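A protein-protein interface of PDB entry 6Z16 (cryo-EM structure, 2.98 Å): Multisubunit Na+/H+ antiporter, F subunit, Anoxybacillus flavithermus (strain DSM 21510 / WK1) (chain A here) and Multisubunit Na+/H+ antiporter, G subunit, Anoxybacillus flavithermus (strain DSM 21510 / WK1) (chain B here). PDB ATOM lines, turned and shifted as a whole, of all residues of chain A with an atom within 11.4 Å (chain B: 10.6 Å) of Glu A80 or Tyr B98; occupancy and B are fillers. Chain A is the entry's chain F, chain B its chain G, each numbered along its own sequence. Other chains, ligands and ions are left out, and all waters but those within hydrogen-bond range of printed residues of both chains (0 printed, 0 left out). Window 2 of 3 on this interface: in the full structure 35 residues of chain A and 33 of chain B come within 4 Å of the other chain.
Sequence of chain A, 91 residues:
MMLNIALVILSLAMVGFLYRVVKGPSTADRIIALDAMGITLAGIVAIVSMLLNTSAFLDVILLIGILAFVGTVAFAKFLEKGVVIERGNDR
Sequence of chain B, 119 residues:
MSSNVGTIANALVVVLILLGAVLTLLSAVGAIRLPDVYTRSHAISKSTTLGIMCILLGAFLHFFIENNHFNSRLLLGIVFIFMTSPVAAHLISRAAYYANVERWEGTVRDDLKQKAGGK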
ATOM      1  N   SER A  26      -0.975  -7.439  39.285  1.00  0.00           N
ATOM      2  CA  SER A  26      -0.787  -6.500  38.194  1.00  0.00           C
ATOM      3  C   SER A  26      -2.070  -5.715  37.943  1.00  0.00           C
ATOM      4  O   SER A  26      -3.130  -6.004  38.502  1.00  0.00           O
ATOM      5  CB  SER A  26      -0.350  -7.234  36.932  1.00  0.00           C
ATOM      6  OG  SER A  26      -1.373  -8.104  36.482  1.00  0.00           O
ATOM      7  N   THR A  27      -1.965  -4.705  37.084  1.00  0.00           N
ATOM      8  CA  THR A  27      -3.121  -3.876  36.762  1.00  0.00           C
ATOM      9  C   THR A  27      -4.013  -4.551  35.723  1.00  0.00           C
ATOM     10  O   THR A  27      -5.242  -4.357  35.732  1.00  0.00           O
ATOM     11  CB  THR A  27      -2.634  -2.515  36.264  1.00  0.00           C
ATOM     12  OG1 THR A  27      -1.642  -2.015  37.167  1.00  0.00           O
ATOM     13  CG2 THR A  27      -3.765  -1.515  36.227  1.00  0.00           C
ATOM     14  N   ALA A  28      -3.408  -5.395  34.879  1.00  0.00           N
ATOM     15  CA  ALA A  28      -4.095  -5.984  33.732  1.00  0.00           C
ATOM     16  C   ALA A  28      -5.238  -6.903  34.153  1.00  0.00           C
ATOM     17  O   ALA A  28      -6.271  -6.966  33.472  1.00  0.00           O
ATOM     18  CB  ALA A  28      -3.086  -6.743  32.874  1.00  0.00           C
ATOM     19  N   ILE A  31      -8.114  -4.713  34.842  1.00  0.00           N
ATOM     20  CA  ILE A  31      -8.701  -4.175  33.615  1.00  0.00           C
ATOM     21  C   ILE A  31      -9.616  -5.200  32.954  1.00  0.00           C
ATOM     22  O   ILE A  31     -10.736  -4.875  32.530  1.00  0.00           O
ATOM     23  CB  ILE A  31      -7.597  -3.732  32.646  1.00  0.00           C
ATOM     24  CG1 ILE A  31      -6.663  -2.754  33.316  1.00  0.00           C
ATOM     25  CG2 ILE A  31      -8.206  -3.024  31.468  1.00  0.00           C
ATOM     26  CD1 ILE A  31      -5.395  -2.666  32.593  1.00  0.00           C
ATOM     27  N   GLY A  71     -13.103   2.206  26.408  1.00  0.00           N
ATOM     28  CA  GLY A  71     -12.358   2.332  27.654  1.00  0.00           C
ATOM     29  C   GLY A  71     -11.200   1.357  27.769  1.00  0.00           C
ATOM     30  O   GLY A  71     -10.112   1.723  28.233  1.00  0.00           O
ATOM     31  N   THR A  72     -11.397   0.113  27.317  1.00  0.00           N
ATOM     32  CA  THR A  72     -10.314  -0.860  27.416  1.00  0.00           C
ATOM     33  C   THR A  72      -9.184  -0.560  26.440  1.00  0.00           C
ATOM     34  O   THR A  72      -8.011  -0.727  26.795  1.00  0.00           O
ATOM     35  CB  THR A  72     -10.839  -2.277  27.210  1.00  0.00           C
ATOM     36  OG1 THR A  72     -11.613  -2.340  26.008  1.00  0.00           O
ATOM     37  CG2 THR A  72     -11.660  -2.706  28.400  1.00  0.00           C
ATOM     38  N   VAL A  73      -9.500  -0.093  25.225  1.00  0.00           N
ATOM     39  CA  VAL A  73      -8.400   0.248  24.322  1.00  0.00           C
ATOM     40  C   VAL A  73      -7.692   1.514  24.791  1.00  0.00           C
ATOM     41  O   VAL A  73      -6.474   1.645  24.607  1.00  0.00           O
ATOM     42  CB  VAL A  73      -8.863   0.357  22.853  1.00  0.00           C
ATOM     43  CG1 VAL A  73      -9.484  -0.926  22.412  1.00  0.00           C
ATOM     44  CG2 VAL A  73      -9.819   1.501  22.622  1.00  0.00           C
ATOM     45  N   ALA A  74      -8.407   2.415  25.482  1.00  0.00           N
ATOM     46  CA  ALA A  74      -7.773   3.608  26.034  1.00  0.00           C
ATOM     47  C   ALA A  74      -6.783   3.254  27.137  1.00  0.00           C
ATOM     48  O   ALA A  74      -5.632   3.711  27.120  1.00  0.00           O
ATOM     49  CB  ALA A  74      -8.837   4.567  26.556  1.00  0.00           C
ATOM     50  N   PHE A  75      -7.186   2.395  28.078  1.00  0.00           N
ATOM     51  CA  PHE A  75      -6.254   2.105  29.161  1.00  0.00           C
ATOM     52  C   PHE A  75      -5.143   1.152  28.716  1.00  0.00           C
ATOM     53  O   PHE A  75      -4.026   1.227  29.244  1.00  0.00           O
ATOM     54  CB  PHE A  75      -6.977   1.547  30.387  1.00  0.00           C
ATOM     55  CG  PHE A  75      -6.206   1.743  31.658  1.00  0.00           C
ATOM     56  CD1 PHE A  75      -6.310   2.928  32.366  1.00  0.00           C
ATOM     57  CD2 PHE A  75      -5.310   0.793  32.096  1.00  0.00           C
ATOM     58  CE1 PHE A  75      -5.579   3.130  33.518  1.00  0.00           C
ATOM     59  CE2 PHE A  75      -4.568   0.982  33.251  1.00  0.00           C
ATOM     60  CZ  PHE A  75      -4.703   2.160  33.960  1.00  0.00           C
ATOM     61  N   ALA A  76      -5.414   0.275  27.741  1.00  0.00           N
ATOM     62  CA  ALA A  76      -4.351  -0.542  27.169  1.00  0.00           C
ATOM     63  C   ALA A  76      -3.344   0.301  26.410  1.00  0.00           C
ATOM     64  O   ALA A  76      -2.164  -0.055  26.354  1.00  0.00           O
ATOM     65  CB  ALA A  76      -4.939  -1.592  26.237  1.00  0.00           C
ATOM     66  N   LYS A  77      -3.788   1.401  25.803  1.00  0.00           N
ATOM     67  CA  LYS A  77      -2.834   2.343  25.240  1.00  0.00           C
ATOM     68  C   LYS A  77      -2.082   3.081  26.340  1.00  0.00           C
ATOM     69  O   LYS A  77      -0.910   3.433  26.157  1.00  0.00           O
ATOM     70  CB  LYS A  77      -3.562   3.313  24.305  1.00  0.00           C
ATOM     71  CG  LYS A  77      -2.663   4.294  23.577  1.00  0.00           C
ATOM     72  CD  LYS A  77      -1.716   3.587  22.627  1.00  0.00           C
ATOM     73  CE  LYS A  77      -0.767   4.572  21.968  1.00  0.00           C
ATOM     74  NZ  LYS A  77      -1.473   5.526  21.073  1.00  0.00           N
ATOM     75  N   PHE A  78      -2.724   3.289  27.497  1.00  0.00           N
ATOM     76  CA  PHE A  78      -2.050   3.988  28.591  1.00  0.00           C
ATOM     77  C   PHE A  78      -0.920   3.169  29.202  1.00  0.00           C
ATOM     78  O   PHE A  78       0.135   3.725  29.532  1.00  0.00           O
ATOM     79  CB  PHE A  78      -3.030   4.389  29.689  1.00  0.00           C
ATOM     80  CG  PHE A  78      -2.351   4.986  30.879  1.00  0.00           C
ATOM     81  CD1 PHE A  78      -1.660   6.180  30.760  1.00  0.00           C
ATOM     82  CD2 PHE A  78      -2.389   4.357  32.109  1.00  0.00           C
ATOM     83  CE1 PHE A  78      -1.006   6.729  31.840  1.00  0.00           C
ATOM     84  CE2 PHE A  78      -1.746   4.907  33.200  1.00  0.00           C
ATOM     85  CZ  PHE A  78      -1.054   6.097  33.064  1.00  0.00           C
ATOM     86  N   LEU A  79      -1.116   1.859  29.381  1.00  0.00           N
ATOM     87  CA  LEU A  79      -0.058   1.041  29.974  1.00  0.00           C
ATOM     88  C   LEU A  79       1.148   0.906  29.057  1.00  0.00           C
ATOM     89  O   LEU A  79       2.261   0.655  29.529  1.00  0.00           O
ATOM     90  CB  LEU A  79      -0.567  -0.353  30.312  1.00  0.00           C
ATOM     91  CG  LEU A  79      -1.610  -0.488  31.404  1.00  0.00           C
ATOM     92  CD1 LEU A  79      -1.956  -1.943  31.518  1.00  0.00           C
ATOM     93  CD2 LEU A  79      -1.074   0.045  32.708  1.00  0.00           C
ATOM     94  N   GLU A  80       0.949   1.066  27.756  1.00  0.00           N
ATOM     95  CA  GLU A  80       2.019   0.920  26.779  1.00  0.00           C
ATOM     96  C   GLU A  80       2.601   2.293  26.472  1.00  0.00           C
ATOM     97  O   GLU A  80       2.005   3.081  25.731  1.00  0.00           O
ATOM     98  CB  GLU A  80       1.499   0.232  25.523  1.00  0.00           C
ATOM     99  CG  GLU A  80       2.535   0.036  24.427  1.00  0.00           C
ATOM    100  CD  GLU A  80       3.641  -0.924  24.819  1.00  0.00           C
ATOM    101  OE1 GLU A  80       3.396  -1.794  25.676  1.00  0.00           O
ATOM    102  OE2 GLU A  80       4.754  -0.814  24.263  1.00  0.00           O
ATOM    103  N   LYS A  81       3.753   2.581  27.089  1.00  0.00           N
ATOM    104  CA  LYS A  81       4.661   3.667  26.704  1.00  0.00           C
ATOM    105  C   LYS A  81       4.026   5.049  26.849  1.00  0.00           C
ATOM    106  O   LYS A  81       4.162   5.907  25.975  1.00  0.00           O
ATOM    107  CB  LYS A  81       5.202   3.452  25.287  1.00  0.00           C
ATOM    108  CG  LYS A  81       6.140   2.256  25.187  1.00  0.00           C
ATOM    109  CD  LYS A  81       6.693   2.050  23.784  1.00  0.00           C
ATOM    110  CE  LYS A  81       7.624   0.840  23.743  1.00  0.00           C
ATOM    111  NZ  LYS A  81       8.168   0.554  22.386  1.00  0.00           N
ATOM    112  N   GLY A  82       3.327   5.269  27.959  1.00  0.00           N
ATOM    113  CA  GLY A  82       2.938   6.616  28.321  1.00  0.00           C
ATOM    114  C   GLY A  82       1.572   7.094  27.874  1.00  0.00           C
ATOM    115  O   GLY A  82       0.570   6.858  28.550  1.00  0.00           O
ATOM    116  N   VAL A  83       1.539   7.795  26.737  1.00  0.00           N
ATOM    117  CA  VAL A  83       0.375   8.585  26.342  1.00  0.00           C
ATOM    118  C   VAL A  83      -0.774   7.691  25.884  1.00  0.00           C
ATOM    119  O   VAL A  83      -0.585   6.553  25.443  1.00  0.00           O
ATOM    120  CB  VAL A  83       0.776   9.575  25.236  1.00  0.00           C
ATOM    121  CG1 VAL A  83       1.824  10.532  25.744  1.00  0.00           C
ATOM    122  CG2 VAL A  83       1.316   8.827  24.029  1.00  0.00           C
ATOM    123  N   VAL A  84      -1.991   8.224  25.998  1.00  0.00           N
ATOM    124  CA  VAL A  84      -3.138   7.624  25.324  1.00  0.00           C
ATOM    125  C   VAL A  84      -3.402   8.277  23.972  1.00  0.00           C
ATOM    126  O   VAL A  84      -4.112   7.694  23.141  1.00  0.00           O
ATOM    127  CB  VAL A  84      -4.423   7.705  26.168  1.00  0.00           C
ATOM    128  CG1 VAL A  84      -4.239   7.011  27.470  1.00  0.00           C
ATOM    129  CG2 VAL A  84      -4.828   9.140  26.412  1.00  0.00           C
ATOM    130  N   ILE A  85      -2.872   9.477  23.740  1.00  0.00           N
ATOM    131  CA  ILE A  85      -3.046  10.227  22.500  1.00  0.00           C
ATOM    132  C   ILE A  85      -1.693  10.822  22.145  1.00  0.00           C
ATOM    133  O   ILE A  85      -1.139  11.609  22.919  1.00  0.00           O
ATOM    134  CB  ILE A  85      -4.103  11.340  22.626  1.00  0.00           C
ATOM    135  CG1 ILE A  85      -5.504  10.752  22.812  1.00  0.00           C
ATOM    136  CG2 ILE A  85      -4.062  12.249  21.419  1.00  0.00           C
ATOM    137  CD1 ILE A  85      -6.539  11.754  23.233  1.00  0.00           C
ATOM    138  N   GLU A  86      -1.152  10.446  20.991  1.00  0.00           N
ATOM    139  CA  GLU A  86       0.172  10.910  20.623  1.00  0.00           C
ATOM    140  C   GLU A  86       0.124  12.360  20.152  1.00  0.00           C
ATOM    141  O   GLU A  86      -0.939  12.935  19.914  1.00  0.00           O
ATOM    142  CB  GLU A  86       0.773  10.029  19.530  1.00  0.00           C
ATOM    143  CG  GLU A  86       1.065   8.610  19.965  1.00  0.00           C
ATOM    144  CD  GLU A  86       1.632   7.768  18.844  1.00  0.00           C
ATOM    145  OE1 GLU A  86       1.720   8.275  17.706  1.00  0.00           O
ATOM    146  OE2 GLU A  86       1.980   6.596  19.097  1.00  0.00           O
ATOM    147  N   VAL B  37      -2.142 -13.948  34.392  1.00  0.00           N
ATOM    148  CA  VAL B  37      -2.972 -12.980  33.678  1.00  0.00           C
ATOM    149  C   VAL B  37      -3.420 -13.538  32.324  1.00  0.00           C
ATOM    150  O   VAL B  37      -4.543 -13.272  31.871  1.00  0.00           O
ATOM    151  CB  VAL B  37      -2.219 -11.636  33.555  1.00  0.00           C
ATOM    152  CG1 VAL B  37      -0.894 -11.795  32.822  1.00  0.00           C
ATOM    153  CG2 VAL B  37      -3.075 -10.576  32.876  1.00  0.00           C
ATOM    154  N   TYR B  38      -2.604 -14.390  31.704  1.00  0.00           N
ATOM    155  CA  TYR B  38      -2.888 -14.845  30.350  1.00  0.00           C
ATOM    156  C   TYR B  38      -3.931 -15.957  30.338  1.00  0.00           C
ATOM    157  O   TYR B  38      -4.783 -16.005  29.442  1.00  0.00           O
ATOM    158  CB  TYR B  38      -1.596 -15.320  29.704  1.00  0.00           C
ATOM    159  CG  TYR B  38      -0.492 -14.309  29.790  1.00  0.00           C
ATOM    160  CD1 TYR B  38      -0.477 -13.195  28.971  1.00  0.00           C
ATOM    161  CD2 TYR B  38       0.550 -14.480  30.686  1.00  0.00           C
ATOM    162  CE1 TYR B  38       0.545 -12.271  29.051  1.00  0.00           C
ATOM    163  CE2 TYR B  38       1.574 -13.565  30.770  1.00  0.00           C
ATOM    164  CZ  TYR B  38       1.567 -12.463  29.952  1.00  0.00           C
ATOM    165  OH  TYR B  38       2.585 -11.553  30.037  1.00  0.00           O
ATOM    166  N   HIS B  90      -6.633  -9.330  23.596  1.00  0.00           N
ATOM    167  CA  HIS B  90      -5.335  -9.240  22.931  1.00  0.00           C
ATOM    168  C   HIS B  90      -4.563  -7.998  23.353  1.00  0.00           C
ATOM    169  O   HIS B  90      -3.355  -8.069  23.612  1.00  0.00           O
ATOM    170  CB  HIS B  90      -5.526  -9.238  21.415  1.00  0.00           C
ATOM    171  CG  HIS B  90      -4.263  -8.993  20.650  1.00  0.00           C
ATOM    172  ND1 HIS B  90      -3.840  -7.731  20.295  1.00  0.00           N
ATOM    173  CD2 HIS B  90      -3.322  -9.846  20.187  1.00  0.00           C
ATOM    174  CE1 HIS B  90      -2.698  -7.818  19.639  1.00  0.00           C
ATOM    175  NE2 HIS B  90      -2.361  -9.091  19.561  1.00  0.00           N
ATOM    176  N   LEU B  91      -5.242  -6.853  23.425  1.00  0.00           N
ATOM    177  CA  LEU B  91      -4.558  -5.613  23.777  1.00  0.00           C
ATOM    178  C   LEU B  91      -4.115  -5.603  25.233  1.00  0.00           C
ATOM    179  O   LEU B  91      -2.996  -5.168  25.536  1.00  0.00           O
ATOM    180  CB  LEU B  91      -5.454  -4.419  23.469  1.00  0.00           C
ATOM    181  CG  LEU B  91      -5.556  -4.157  21.971  1.00  0.00           C
ATOM    182  CD1 LEU B  91      -6.644  -3.169  21.694  1.00  0.00           C
ATOM    183  CD2 LEU B  91      -4.226  -3.641  21.445  1.00  0.00           C
ATOM    184  N   ILE B  92      -4.957  -6.110  26.143  1.00  0.00           N
ATOM    185  CA  ILE B  92      -4.547  -6.150  27.548  1.00  0.00           C
ATOM    186  C   ILE B  92      -3.427  -7.166  27.750  1.00  0.00           C
ATOM    187  O   ILE B  92      -2.520  -6.944  28.559  1.00  0.00           O
ATOM    188  CB  ILE B  92      -5.727  -6.454  28.489  1.00  0.00           C
ATOM    189  CG1 ILE B  92      -6.932  -5.571  28.195  1.00  0.00           C
ATOM    190  CG2 ILE B  92      -5.332  -6.159  29.912  1.00  0.00           C
ATOM    191  CD1 ILE B  92      -6.688  -4.107  28.300  1.00  0.00           C
ATOM    192  N   SER B  93      -3.432  -8.265  26.992  1.00  0.00           N
ATOM    193  CA  SER B  93      -2.373  -9.256  27.144  1.00  0.00           C
ATOM    194  C   SER B  93      -1.048  -8.759  26.577  1.00  0.00           C
ATOM    195  O   SER B  93       0.010  -9.031  27.154  1.00  0.00           O
ATOM    196  CB  SER B  93      -2.788 -10.564  26.483  1.00  0.00           C
ATOM    197  OG  SER B  93      -3.907 -11.119  27.147  1.00  0.00           O
ATOM    198  N   ARG B  94      -1.078  -8.006  25.472  1.00  0.00           N
ATOM    199  CA  ARG B  94       0.165  -7.419  24.978  1.00  0.00           C
ATOM    200  C   ARG B  94       0.664  -6.329  25.918  1.00  0.00           C
ATOM    201  O   ARG B  94       1.880  -6.184  26.124  1.00  0.00           O
ATOM    202  CB  ARG B  94      -0.009  -6.855  23.567  1.00  0.00           C
ATOM    203  CG  ARG B  94       1.334  -6.486  22.947  1.00  0.00           C
ATOM    204  CD  ARG B  94       1.284  -5.921  21.535  1.00  0.00           C
ATOM    205  NE  ARG B  94       0.706  -4.585  21.475  1.00  0.00           N
ATOM    206  CZ  ARG B  94      -0.368  -4.272  20.763  1.00  0.00           C
ATOM    207  NH1 ARG B  94      -0.967  -5.197  20.031  1.00  0.00           N
ATOM    208  NH2 ARG B  94      -0.830  -3.031  20.764  1.00  0.00           N
ATOM    209  N   ALA B  95      -0.259  -5.569  26.518  1.00  0.00           N
ATOM    210  CA  ALA B  95       0.130  -4.538  27.472  1.00  0.00           C
ATOM    211  C   ALA B  95       0.716  -5.141  28.739  1.00  0.00           C
ATOM    212  O   ALA B  95       1.618  -4.553  29.344  1.00  0.00           O
ATOM    213  CB  ALA B  95      -1.072  -3.661  27.809  1.00  0.00           C
ATOM    214  N   ALA B  96       0.233  -6.314  29.138  1.00  0.00           N
ATOM    215  CA  ALA B  96       0.801  -6.994  30.291  1.00  0.00           C
ATOM    216  C   ALA B  96       2.143  -7.623  29.961  1.00  0.00           C
ATOM    217  O   ALA B  96       3.042  -7.633  30.804  1.00  0.00           O
ATOM    218  CB  ALA B  96      -0.165  -8.055  30.811  1.00  0.00           C
ATOM    219  N   TYR B  97       2.301  -8.155  28.747  1.00  0.00           N
ATOM    220  CA  TYR B  97       3.564  -8.788  28.384  1.00  0.00           C
ATOM    221  C   TYR B  97       4.675  -7.765  28.223  1.00  0.00           C
ATOM    222  O   TYR B  97       5.821  -8.030  28.594  1.00  0.00           O
ATOM    223  CB  TYR B  97       3.415  -9.596  27.100  1.00  0.00           C
ATOM    224  CG  TYR B  97       4.664 -10.357  26.729  1.00  0.00           C
ATOM    225  CD1 TYR B  97       4.999 -11.530  27.384  1.00  0.00           C
ATOM    226  CD2 TYR B  97       5.512  -9.900  25.734  1.00  0.00           C
ATOM    227  CE1 TYR B  97       6.142 -12.232  27.055  1.00  0.00           C
ATOM    228  CE2 TYR B  97       6.661 -10.594  25.396  1.00  0.00           C
ATOM    229  CZ  TYR B  97       6.968 -11.759  26.063  1.00  0.00           C
ATOM    230  OH  TYR B  97       8.102 -12.462  25.738  1.00  0.00           O
ATOM    231  N   TYR B  98       4.364  -6.597  27.668  1.00  0.00           N
ATOM    232  CA  TYR B  98       5.386  -5.571  27.504  1.00  0.00           C
ATOM    233  C   TYR B  98       5.771  -4.882  28.805  1.00  0.00           C
ATOM    234  O   TYR B  98       6.796  -4.194  28.837  1.00  0.00           O
ATOM    235  CB  TYR B  98       4.924  -4.532  26.488  1.00  0.00           C
ATOM    236  CG  TYR B  98       5.131  -4.932  25.047  1.00  0.00           C
ATOM    237  CD1 TYR B  98       6.055  -5.910  24.706  1.00  0.00           C
ATOM    238  CD2 TYR B  98       4.413  -4.322  24.026  1.00  0.00           C
ATOM    239  CE1 TYR B  98       6.256  -6.273  23.393  1.00  0.00           C
ATOM    240  CE2 TYR B  98       4.601  -4.677  22.705  1.00  0.00           C
ATOM    241  CZ  TYR B  98       5.527  -5.649  22.395  1.00  0.00           C
ATOM    242  OH  TYR B  98       5.716  -6.003  21.077  1.00  0.00           O
ATOM    243  N   ALA B  99       4.997  -5.060  29.875  1.00  0.00           N
ATOM    244  CA  ALA B  99       5.321  -4.505  31.180  1.00  0.00           C
ATOM    245  C   ALA B  99       6.276  -5.385  31.982  1.00  0.00           C
ATOM    246  O   ALA B  99       6.415  -5.168  33.191  1.00  0.00           O
ATOM    247  CB  ALA B  99       4.040  -4.267  31.981  1.00  0.00           C
ATOM    248  N   ASN B 100       6.936  -6.351  31.326  1.00  0.00           N
ATOM    249  CA  ASN B 100       7.809  -7.358  31.947  1.00  0.00           C
ATOM    250  C   ASN B 100       7.101  -8.108  33.070  1.00  0.00           C
ATOM    251  O   ASN B 100       7.692  -8.427  34.103  1.00  0.00           O
ATOM    252  CB  ASN B 100       9.119  -6.743  32.442  1.00  0.00           C
ATOM    253  CG  ASN B 100      10.063  -6.396  31.308  1.00  0.00           C
ATOM    254  OD1 ASN B 100      10.217  -7.164  30.359  1.00  0.00           O
ATOM    255  ND2 ASN B 100      10.704  -5.236  31.403  1.00  0.00           N
ATOM    256  N   VAL B 101       5.820  -8.392  32.862  1.00  0.00           N
ATOM    257  CA  VAL B 101       4.989  -9.089  33.834  1.00  0.00           C
ATOM    258  C   VAL B 101       4.857 -10.531  33.378  1.00  0.00           C
ATOM    259  O   VAL B 101       4.385 -10.797  32.267  1.00  0.00           O
ATOM    260  CB  VAL B 101       3.612  -8.428  33.979  1.00  0.00           C
ATOM    261  CG1 VAL B 101       2.704  -9.263  34.861  1.00  0.00           C
ATOM    262  CG2 VAL B 101       3.761  -7.031  34.537  1.00  0.00           C
ATOM    263  N   GLU B 102       5.285 -11.461  34.227  1.00  0.00           N
ATOM    264  CA  GLU B 102       5.103 -12.878  33.952  1.00  0.00           C
ATOM    265  C   GLU B 102       4.858 -13.595  35.268  1.00  0.00           C
ATOM    266  O   GLU B 102       5.459 -13.252  36.291  1.00  0.00           O
ATOM    267  CB  GLU B 102       6.304 -13.478  33.207  1.00  0.00           C
ATOM    268  CG  GLU B 102       7.631 -13.455  33.947  1.00  0.00           C
ATOM    269  CD  GLU B 102       8.741 -14.060  33.125  1.00  0.00           C
ATOM    270  OE1 GLU B 102       8.470 -14.438  31.968  1.00  0.00           O
ATOM    271  OE2 GLU B 102       9.875 -14.171  33.635  1.00  0.00           O
ATOM    272  N   ARG B 109       9.231 -20.602  26.817  1.00  0.00           N
ATOM    273  CA  ARG B 109       8.816 -19.402  26.073  1.00  0.00           C
ATOM    274  C   ARG B 109       9.943 -18.553  25.490  1.00  0.00           C
ATOM    275  O   ARG B 109      11.002 -18.376  26.098  1.00  0.00           O
ATOM    276  CB  ARG B 109       7.955 -18.528  27.002  1.00  0.00           C
ATOM    277  CG  ARG B 109       8.607 -18.124  28.335  1.00  0.00           C
ATOM    278  CD  ARG B 109       9.253 -16.737  28.314  1.00  0.00           C
ATOM    279  NE  ARG B 109       9.828 -16.376  29.604  1.00  0.00           N
ATOM    280  CZ  ARG B 109      10.548 -15.279  29.817  1.00  0.00           C
ATOM    281  NH1 ARG B 109      10.771 -14.425  28.828  1.00  0.00           N
ATOM    282  NH2 ARG B 109      11.032 -15.030  31.025  1.00  0.00           N
ATOM    283  N   ASP B 110       9.691 -18.035  24.292  1.00  0.00           N
ATOM    284  CA  ASP B 110      10.564 -17.101  23.601  1.00  0.00           C
ATOM    285  C   ASP B 110      10.046 -15.675  23.761  1.00  0.00           C
ATOM    286  O   ASP B 110       8.887 -15.451  24.123  1.00  0.00           O
ATOM    287  CB  ASP B 110      10.686 -17.470  22.117  1.00  0.00           C
ATOM    288  CG  ASP B 110       9.337 -17.613  21.431  1.00  0.00           C
ATOM    289  OD1 ASP B 110       8.291 -17.537  22.107  1.00  0.00           O
ATOM    290  OD2 ASP B 110       9.324 -17.813  20.203  1.00  0.00           O
ATOM    291  N   ASP B 111      10.922 -14.714  23.486  1.00  0.00           N
ATOM    292  CA  ASP B 111      10.614 -13.301  23.686  1.00  0.00           C
ATOM    293  C   ASP B 111       9.528 -12.800  22.731  1.00  0.00           C
ATOM    294  O   ASP B 111       8.345 -12.787  23.075  1.00  0.00           O
ATOM    295  CB  ASP B 111      11.882 -12.456  23.524  1.00  0.00           C
ATOM    296  CG  ASP B 111      12.886 -12.698  24.631  1.00  0.00           C
ATOM    297  OD1 ASP B 111      12.465 -13.060  25.750  1.00  0.00           O
ATOM    298  OD2 ASP B 111      14.097 -12.520  24.384  1.00  0.00           O
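Printed residues of chain B within 4 Å of Ile A31: Ile B92.
Of the printed residues of chain B, Val A73 touches Leu B91 (3.7 Å).
Printed residues of chain B within 4 Å of Ala A76: Leu B91 and Ile B92.
No residue of chain B comes within 4 Å of Lys A77.
No residue of chain B comes within 4 Å of Lys A81.
Val A84 touches none of the printed residues of chain B.
Printed residues of chain A within 4 Å of Val B37: Ala A28.
Of the printed residues of chain A, Leu B91 touches Val A73 and Ala A76.
Ala B96 touches just one residue of chain A: Ala A28 (3.8 Å).
No residue of chain A comes within 4 Å of Tyr B97.
Of chain A, only Glu A80 (3.2 Å) comes within 4 Å of Tyr B98.
No residue of chain A comes within 4 Å of Ala B99.
No residue of chain A comes within 4 Å of Asn B100.
The nearest printed residue of chain B that does not touch Thr A72 is Leu B91 (5.6 Å).
Among the printed residues, merely in contact across the chains: Glu A80 with Tyr B98, Ile A31 with Ile B92, Val A73 with Leu B91, Ala A76 with Ile B92, Ala A28 with Ile B92, Ala A28 with Ala B96, Ala A28 with Val B37, Thr A72 with Ile B92 and Ala A76 with Leu B91.
Hydrophobic or aromatic side chains of chain B within 4 Å of the printed part of chain A: Val B37, Leu B91, Ile B92, Ala B96 and Tyr B98.
Of the 20 printed residues of chain A, 6 touch a printed residue of chain B.
Hydrophobic or aromatic side chains of chain A within 4 Å of the printed part of chain B: Ala A28, Ile A31, Val A73 and Ala A76.
Among the printed residues, 9 pairs touch across the chains.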
